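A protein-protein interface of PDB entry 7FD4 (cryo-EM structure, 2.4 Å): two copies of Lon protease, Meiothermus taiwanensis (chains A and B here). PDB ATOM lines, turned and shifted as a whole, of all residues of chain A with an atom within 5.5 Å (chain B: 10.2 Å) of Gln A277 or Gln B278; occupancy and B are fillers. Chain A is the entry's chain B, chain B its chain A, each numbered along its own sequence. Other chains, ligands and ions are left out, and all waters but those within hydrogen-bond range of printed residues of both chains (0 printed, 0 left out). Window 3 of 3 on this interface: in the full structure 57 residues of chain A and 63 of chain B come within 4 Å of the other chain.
NE2 of Gln A277 is in hydrogen-bond range of O of Gln B278 (3.0 Å).
The side-chain amide oxygen (OE1) of Gln B278 lies close to the backbone carbonyl oxygen (O) of Met A276.
OG1 of Thr B284 is in hydrogen-bond range of OE2 of Glu A282, at 3.5 Å.
Among the printed residues, merely in contact across the chains: Arg A275 with Gln B278, Gln A277 with Gly B279 and Glu A282 with Pro B281.
Of the printed residues of chain B, Met A276 touches Gln B278.
Printed residues of chain B within 4 Å of Gln A277: Gln B278 and Gly B279.
No residue of chain B comes within 4 Å of Gln A278.
No residue of chain B comes within 4 Å of Gly A279.
Of the printed residues of chain B, Glu A282 touches Pro B281 (3.4 Å) and Thr B284 (3.5 Å).
Gln B278 touches just these residues of chain A: Arg A275 (3.9 Å), Met A276 (3.0 Å) and Gln A277 (3.0 Å).
Of the printed residues of chain A, Pro B281 touches Glu A282.
Of the printed residues of chain A, Thr B284 touches Glu A282.
The nearest residue of chain B that does not touch Gln A277 is Pro B281 (4.3 Å).
Of the 8 printed residues of chain A, 4 touch a printed residue of chain B.
Printed residues of chain A that touch a printed residue of chain B: Arg A275, Met A276, Gln A277 and Glu A282.
Among the printed residues, no Asp or Glu carboxylate lies within 4 Å of a Lys or Arg side-chain nitrogen of the other chain.
Arg A275 touches Gln B278, but with the chains exchanged Gln A278 does not touch Arg B275 (13.0 Å).
Met A276 touches Gln B278, but with the chains exchanged Gln A278 does not touch Met B276 (12.1 Å).
Gln A277 touches Gln B278, but with the chains exchanged Gln A278 does not touch Gln B277 (9.9 Å).
Gln A277 touches Gly B279, but with the chains exchanged Gly A279 does not touch Gln B277 (13.0 Å).
Of the 6 pairs that touch across the chains among the printed residues, none has its exchanged pair printed and touching as well.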
ATOM      1  N   ARG A 275     -26.518  29.672   4.034  1.00  0.00           N
ATOM      2  CA  ARG A 275     -25.610  29.118   3.041  1.00  0.00           C
ATOM      3  C   ARG A 275     -26.315  28.468   1.864  1.00  0.00           C
ATOM      4  O   ARG A 275     -25.692  28.306   0.813  1.00  0.00           O
ATOM      5  CB  ARG A 275     -24.689  28.073   3.671  1.00  0.00           C
ATOM      6  CG  ARG A 275     -23.708  28.621   4.669  1.00  0.00           C
ATOM      7  CD  ARG A 275     -22.809  27.517   5.171  1.00  0.00           C
ATOM      8  NE  ARG A 275     -21.883  28.004   6.179  1.00  0.00           N
ATOM      9  CZ  ARG A 275     -22.119  27.954   7.483  1.00  0.00           C
ATOM     10  NH1 ARG A 275     -21.227  28.424   8.341  1.00  0.00           N
ATOM     11  NH2 ARG A 275     -23.245  27.418   7.929  1.00  0.00           N
ATOM     12  N   MET A 276     -27.578  28.081   2.018  1.00  0.00           N
ATOM     13  CA  MET A 276     -28.281  27.351   0.978  1.00  0.00           C
ATOM     14  C   MET A 276     -28.582  28.256  -0.208  1.00  0.00           C
ATOM     15  O   MET A 276     -28.590  29.484  -0.102  1.00  0.00           O
ATOM     16  CB  MET A 276     -29.586  26.778   1.515  1.00  0.00           C
ATOM     17  CG  MET A 276     -29.415  25.751   2.591  1.00  0.00           C
ATOM     18  SD  MET A 276     -30.999  25.166   3.178  1.00  0.00           S
ATOM     19  CE  MET A 276     -30.496  24.088   4.499  1.00  0.00           C
ATOM     20  N   GLN A 277     -28.817  27.630  -1.355  1.00  0.00           N
ATOM     21  CA  GLN A 277     -29.231  28.381  -2.529  1.00  0.00           C
ATOM     22  C   GLN A 277     -30.659  28.857  -2.365  1.00  0.00           C
ATOM     23  O   GLN A 277     -31.533  28.106  -1.927  1.00  0.00           O
ATOM     24  CB  GLN A 277     -29.117  27.535  -3.789  1.00  0.00           C
ATOM     25  CG  GLN A 277     -27.705  27.286  -4.234  1.00  0.00           C
ATOM     26  CD  GLN A 277     -27.646  26.439  -5.480  1.00  0.00           C
ATOM     27  OE1 GLN A 277     -28.667  25.936  -5.950  1.00  0.00           O
ATOM     28  NE2 GLN A 277     -26.451  26.288  -6.037  1.00  0.00           N
ATOM     29  N   GLN A 278     -30.889  30.119  -2.703  1.00  0.00           N
ATOM     30  CA  GLN A 278     -32.246  30.630  -2.744  1.00  0.00           C
ATOM     31  C   GLN A 278     -32.976  29.953  -3.888  1.00  0.00           C
ATOM     32  O   GLN A 278     -32.577  30.056  -5.050  1.00  0.00           O
ATOM     33  CB  GLN A 278     -32.249  32.146  -2.888  1.00  0.00           C
ATOM     34  CG  GLN A 278     -31.618  32.821  -1.694  1.00  0.00           C
ATOM     35  CD  GLN A 278     -32.361  32.521  -0.402  1.00  0.00           C
ATOM     36  OE1 GLN A 278     -33.591  32.502  -0.369  1.00  0.00           O
ATOM     37  NE2 GLN A 278     -31.615  32.265   0.666  1.00  0.00           N
ATOM     38  N   GLY A 279     -34.042  29.261  -3.540  1.00  0.00           N
ATOM     39  CA  GLY A 279     -34.561  28.149  -4.297  1.00  0.00           C
ATOM     40  C   GLY A 279     -35.681  27.671  -3.412  1.00  0.00           C
ATOM     41  O   GLY A 279     -36.507  28.513  -3.059  1.00  0.00           O
ATOM     42  N   SER A 280     -35.775  26.406  -2.999  1.00  0.00           N
ATOM     43  CA  SER A 280     -34.877  25.256  -3.143  1.00  0.00           C
ATOM     44  C   SER A 280     -35.781  24.270  -2.449  1.00  0.00           C
ATOM     45  O   SER A 280     -36.614  24.693  -1.660  1.00  0.00           O
ATOM     46  CB  SER A 280     -33.533  25.388  -2.407  1.00  0.00           C
ATOM     47  OG  SER A 280     -32.694  24.278  -2.632  1.00  0.00           O
ATOM     48  N   GLU A 282     -34.845  22.370  -0.120  1.00  0.00           N
ATOM     49  CA  GLU A 282     -34.314  22.245   1.223  1.00  0.00           C
ATOM     50  C   GLU A 282     -34.188  23.566   1.957  1.00  0.00           C
ATOM     51  O   GLU A 282     -33.920  23.553   3.159  1.00  0.00           O
ATOM     52  CB  GLU A 282     -32.939  21.574   1.170  1.00  0.00           C
ATOM     53  CG  GLU A 282     -31.944  22.404   0.391  1.00  0.00           C
ATOM     54  CD  GLU A 282     -30.643  21.688   0.118  1.00  0.00           C
ATOM     55  OE1 GLU A 282     -30.514  20.502   0.488  1.00  0.00           O
ATOM     56  OE2 GLU A 282     -29.743  22.317  -0.471  1.00  0.00           O
ATOM     57  N   ALA A 283     -34.352  24.694   1.282  1.00  0.00           N
ATOM     58  CA  ALA A 283     -34.381  25.979   1.958  1.00  0.00           C
ATOM     59  C   ALA A 283     -35.760  26.323   2.483  1.00  0.00           C
ATOM     60  O   ALA A 283     -35.874  27.006   3.507  1.00  0.00           O
ATOM     61  CB  ALA A 283     -33.912  27.084   1.018  1.00  0.00           C
ATOM     62  N   LEU B 237     -11.975  29.651  -3.560  1.00  0.00           N
ATOM     63  CA  LEU B 237     -13.357  29.201  -3.548  1.00  0.00           C
ATOM     64  C   LEU B 237     -14.046  29.463  -2.222  1.00  0.00           C
ATOM     65  O   LEU B 237     -15.275  29.360  -2.151  1.00  0.00           O
ATOM     66  CB  LEU B 237     -13.460  27.709  -3.851  1.00  0.00           C
ATOM     67  CG  LEU B 237     -13.674  27.281  -5.294  1.00  0.00           C
ATOM     68  CD1 LEU B 237     -14.921  27.913  -5.814  1.00  0.00           C
ATOM     69  CD2 LEU B 237     -12.545  27.658  -6.159  1.00  0.00           C
ATOM     70  N   GLY B 238     -13.303  30.036  -1.275  1.00  0.00           N
ATOM     71  CA  GLY B 238     -13.924  30.420   0.004  1.00  0.00           C
ATOM     72  C   GLY B 238     -13.752  31.892   0.288  1.00  0.00           C
ATOM     73  O   GLY B 238     -13.302  32.611  -0.615  1.00  0.00           O
ATOM     74  N   GLY B 239     -14.157  32.336   1.475  1.00  0.00           N
ATOM     75  CA  GLY B 239     -13.944  33.737   1.881  1.00  0.00           C
ATOM     76  C   GLY B 239     -12.989  33.797   3.057  1.00  0.00           C
ATOM     77  O   GLY B 239     -13.065  34.805   3.782  1.00  0.00           O
ATOM     78  N   ASP B 241     -13.458  31.828   5.151  1.00  0.00           N
ATOM     79  CA  ASP B 241     -14.391  30.983   5.924  1.00  0.00           C
ATOM     80  C   ASP B 241     -14.490  29.886   4.880  1.00  0.00           C
ATOM     81  O   ASP B 241     -14.192  30.195   3.709  1.00  0.00           O
ATOM     82  CB  ASP B 241     -15.701  31.718   6.167  1.00  0.00           C
ATOM     83  CG  ASP B 241     -15.937  32.835   5.166  1.00  0.00           C
ATOM     84  OD1 ASP B 241     -15.460  33.957   5.421  1.00  0.00           O
ATOM     85  OD2 ASP B 241     -16.588  32.572   4.139  1.00  0.00           O
ATOM     86  N   GLY B 242     -14.803  28.656   5.244  1.00  0.00           N
ATOM     87  CA  GLY B 242     -14.688  27.614   4.211  1.00  0.00           C
ATOM     88  C   GLY B 242     -13.213  27.298   4.203  1.00  0.00           C
ATOM     89  O   GLY B 242     -12.774  26.540   3.344  1.00  0.00           O
ATOM     90  N   ARG B 275     -16.831  21.527  -3.091  1.00  0.00           N
ATOM     91  CA  ARG B 275     -17.897  21.929  -4.000  1.00  0.00           C
ATOM     92  C   ARG B 275     -18.737  23.093  -3.467  1.00  0.00           C
ATOM     93  O   ARG B 275     -19.900  23.240  -3.861  1.00  0.00           O
ATOM     94  CB  ARG B 275     -18.758  20.716  -4.289  1.00  0.00           C
ATOM     95  CG  ARG B 275     -19.270  20.050  -3.038  1.00  0.00           C
ATOM     96  CD  ARG B 275     -20.034  18.810  -3.390  1.00  0.00           C
ATOM     97  NE  ARG B 275     -20.627  18.192  -2.219  1.00  0.00           N
ATOM     98  CZ  ARG B 275     -20.038  17.242  -1.510  1.00  0.00           C
ATOM     99  NH1 ARG B 275     -18.850  16.792  -1.869  1.00  0.00           N
ATOM    100  NH2 ARG B 275     -20.646  16.730  -0.457  1.00  0.00           N
ATOM    101  N   MET B 276     -18.156  23.940  -2.620  1.00  0.00           N
ATOM    102  CA  MET B 276     -18.850  24.806  -1.669  1.00  0.00           C
ATOM    103  C   MET B 276     -19.323  26.092  -2.355  1.00  0.00           C
ATOM    104  O   MET B 276     -19.492  26.102  -3.579  1.00  0.00           O
ATOM    105  CB  MET B 276     -17.898  25.058  -0.482  1.00  0.00           C
ATOM    106  CG  MET B 276     -18.499  25.407   0.889  1.00  0.00           C
ATOM    107  SD  MET B 276     -17.218  25.515   2.154  1.00  0.00           S
ATOM    108  CE  MET B 276     -18.170  26.038   3.576  1.00  0.00           C
ATOM    109  N   GLN B 277     -19.605  27.144  -1.573  1.00  0.00           N
ATOM    110  CA  GLN B 277     -19.825  28.509  -2.048  1.00  0.00           C
ATOM    111  C   GLN B 277     -21.080  28.686  -2.894  1.00  0.00           C
ATOM    112  O   GLN B 277     -21.020  28.614  -4.126  1.00  0.00           O
ATOM    113  CB  GLN B 277     -18.595  29.045  -2.792  1.00  0.00           C
ATOM    114  CG  GLN B 277     -18.743  30.501  -3.194  1.00  0.00           C
ATOM    115  CD  GLN B 277     -18.851  31.436  -2.006  1.00  0.00           C
ATOM    116  OE1 GLN B 277     -17.945  31.508  -1.175  1.00  0.00           O
ATOM    117  NE2 GLN B 277     -19.982  32.117  -1.891  1.00  0.00           N
ATOM    118  N   GLN B 278     -22.225  28.830  -2.206  1.00  0.00           N
ATOM    119  CA  GLN B 278     -23.570  29.043  -2.750  1.00  0.00           C
ATOM    120  C   GLN B 278     -23.991  27.788  -3.497  1.00  0.00           C
ATOM    121  O   GLN B 278     -24.161  27.775  -4.722  1.00  0.00           O
ATOM    122  CB  GLN B 278     -23.641  30.308  -3.626  1.00  0.00           C
ATOM    123  CG  GLN B 278     -25.051  30.789  -3.968  1.00  0.00           C
ATOM    124  CD  GLN B 278     -25.841  31.199  -2.741  1.00  0.00           C
ATOM    125  OE1 GLN B 278     -26.720  30.473  -2.291  1.00  0.00           O
ATOM    126  NE2 GLN B 278     -25.533  32.372  -2.197  1.00  0.00           N
ATOM    127  N   GLY B 279     -24.127  26.714  -2.736  1.00  0.00           N
ATOM    128  CA  GLY B 279     -24.297  25.384  -3.271  1.00  0.00           C
ATOM    129  C   GLY B 279     -23.157  24.479  -2.847  1.00  0.00           C
ATOM    130  O   GLY B 279     -22.183  24.905  -2.231  1.00  0.00           O
ATOM    131  N   SER B 280     -23.294  23.201  -3.187  1.00  0.00           N
ATOM    132  CA  SER B 280     -24.418  22.618  -3.901  1.00  0.00           C
ATOM    133  C   SER B 280     -25.502  22.218  -2.900  1.00  0.00           C
ATOM    134  O   SER B 280     -25.349  22.469  -1.714  1.00  0.00           O
ATOM    135  CB  SER B 280     -23.916  21.416  -4.708  1.00  0.00           C
ATOM    136  OG  SER B 280     -23.449  20.393  -3.852  1.00  0.00           O
ATOM    137  N   PRO B 281     -26.614  21.640  -3.358  1.00  0.00           N
ATOM    138  CA  PRO B 281     -27.441  20.845  -2.440  1.00  0.00           C
ATOM    139  C   PRO B 281     -26.750  19.616  -1.873  1.00  0.00           C
ATOM    140  O   PRO B 281     -27.262  19.044  -0.909  1.00  0.00           O
ATOM    141  CB  PRO B 281     -28.639  20.453  -3.305  1.00  0.00           C
ATOM    142  CG  PRO B 281     -28.780  21.580  -4.215  1.00  0.00           C
ATOM    143  CD  PRO B 281     -27.397  22.049  -4.538  1.00  0.00           C
ATOM    144  N   GLU B 282     -25.627  19.179  -2.434  1.00  0.00           N
ATOM    145  CA  GLU B 282     -24.884  18.061  -1.881  1.00  0.00           C
ATOM    146  C   GLU B 282     -23.866  18.494  -0.833  1.00  0.00           C
ATOM    147  O   GLU B 282     -23.531  17.699   0.052  1.00  0.00           O
ATOM    148  CB  GLU B 282     -24.207  17.296  -3.026  1.00  0.00           C
ATOM    149  CG  GLU B 282     -23.493  16.014  -2.643  1.00  0.00           C
ATOM    150  CD  GLU B 282     -24.426  14.947  -2.106  1.00  0.00           C
ATOM    151  OE1 GLU B 282     -25.604  14.902  -2.521  1.00  0.00           O
ATOM    152  OE2 GLU B 282     -23.977  14.158  -1.249  1.00  0.00           O
ATOM    153  N   ALA B 283     -23.399  19.741  -0.878  1.00  0.00           N
ATOM    154  CA  ALA B 283     -22.464  20.211   0.142  1.00  0.00           C
ATOM    155  C   ALA B 283     -23.146  20.379   1.491  1.00  0.00           C
ATOM    156  O   ALA B 283     -22.567  20.048   2.532  1.00  0.00           O
ATOM    157  CB  ALA B 283     -21.831  21.526  -0.297  1.00  0.00           C
ATOM    158  N   THR B 284     -24.384  20.869   1.493  1.00  0.00           N
ATOM    159  CA  THR B 284     -25.085  21.078   2.748  1.00  0.00           C
ATOM    160  C   THR B 284     -25.576  19.778   3.356  1.00  0.00           C
ATOM    161  O   THR B 284     -25.903  19.755   4.542  1.00  0.00           O
ATOM    162  CB  THR B 284     -26.265  22.014   2.547  1.00  0.00           C
ATOM    163  OG1 THR B 284     -27.245  21.367   1.735  1.00  0.00           O
ATOM    164  CG2 THR B 284     -25.811  23.273   1.845  1.00  0.00           C
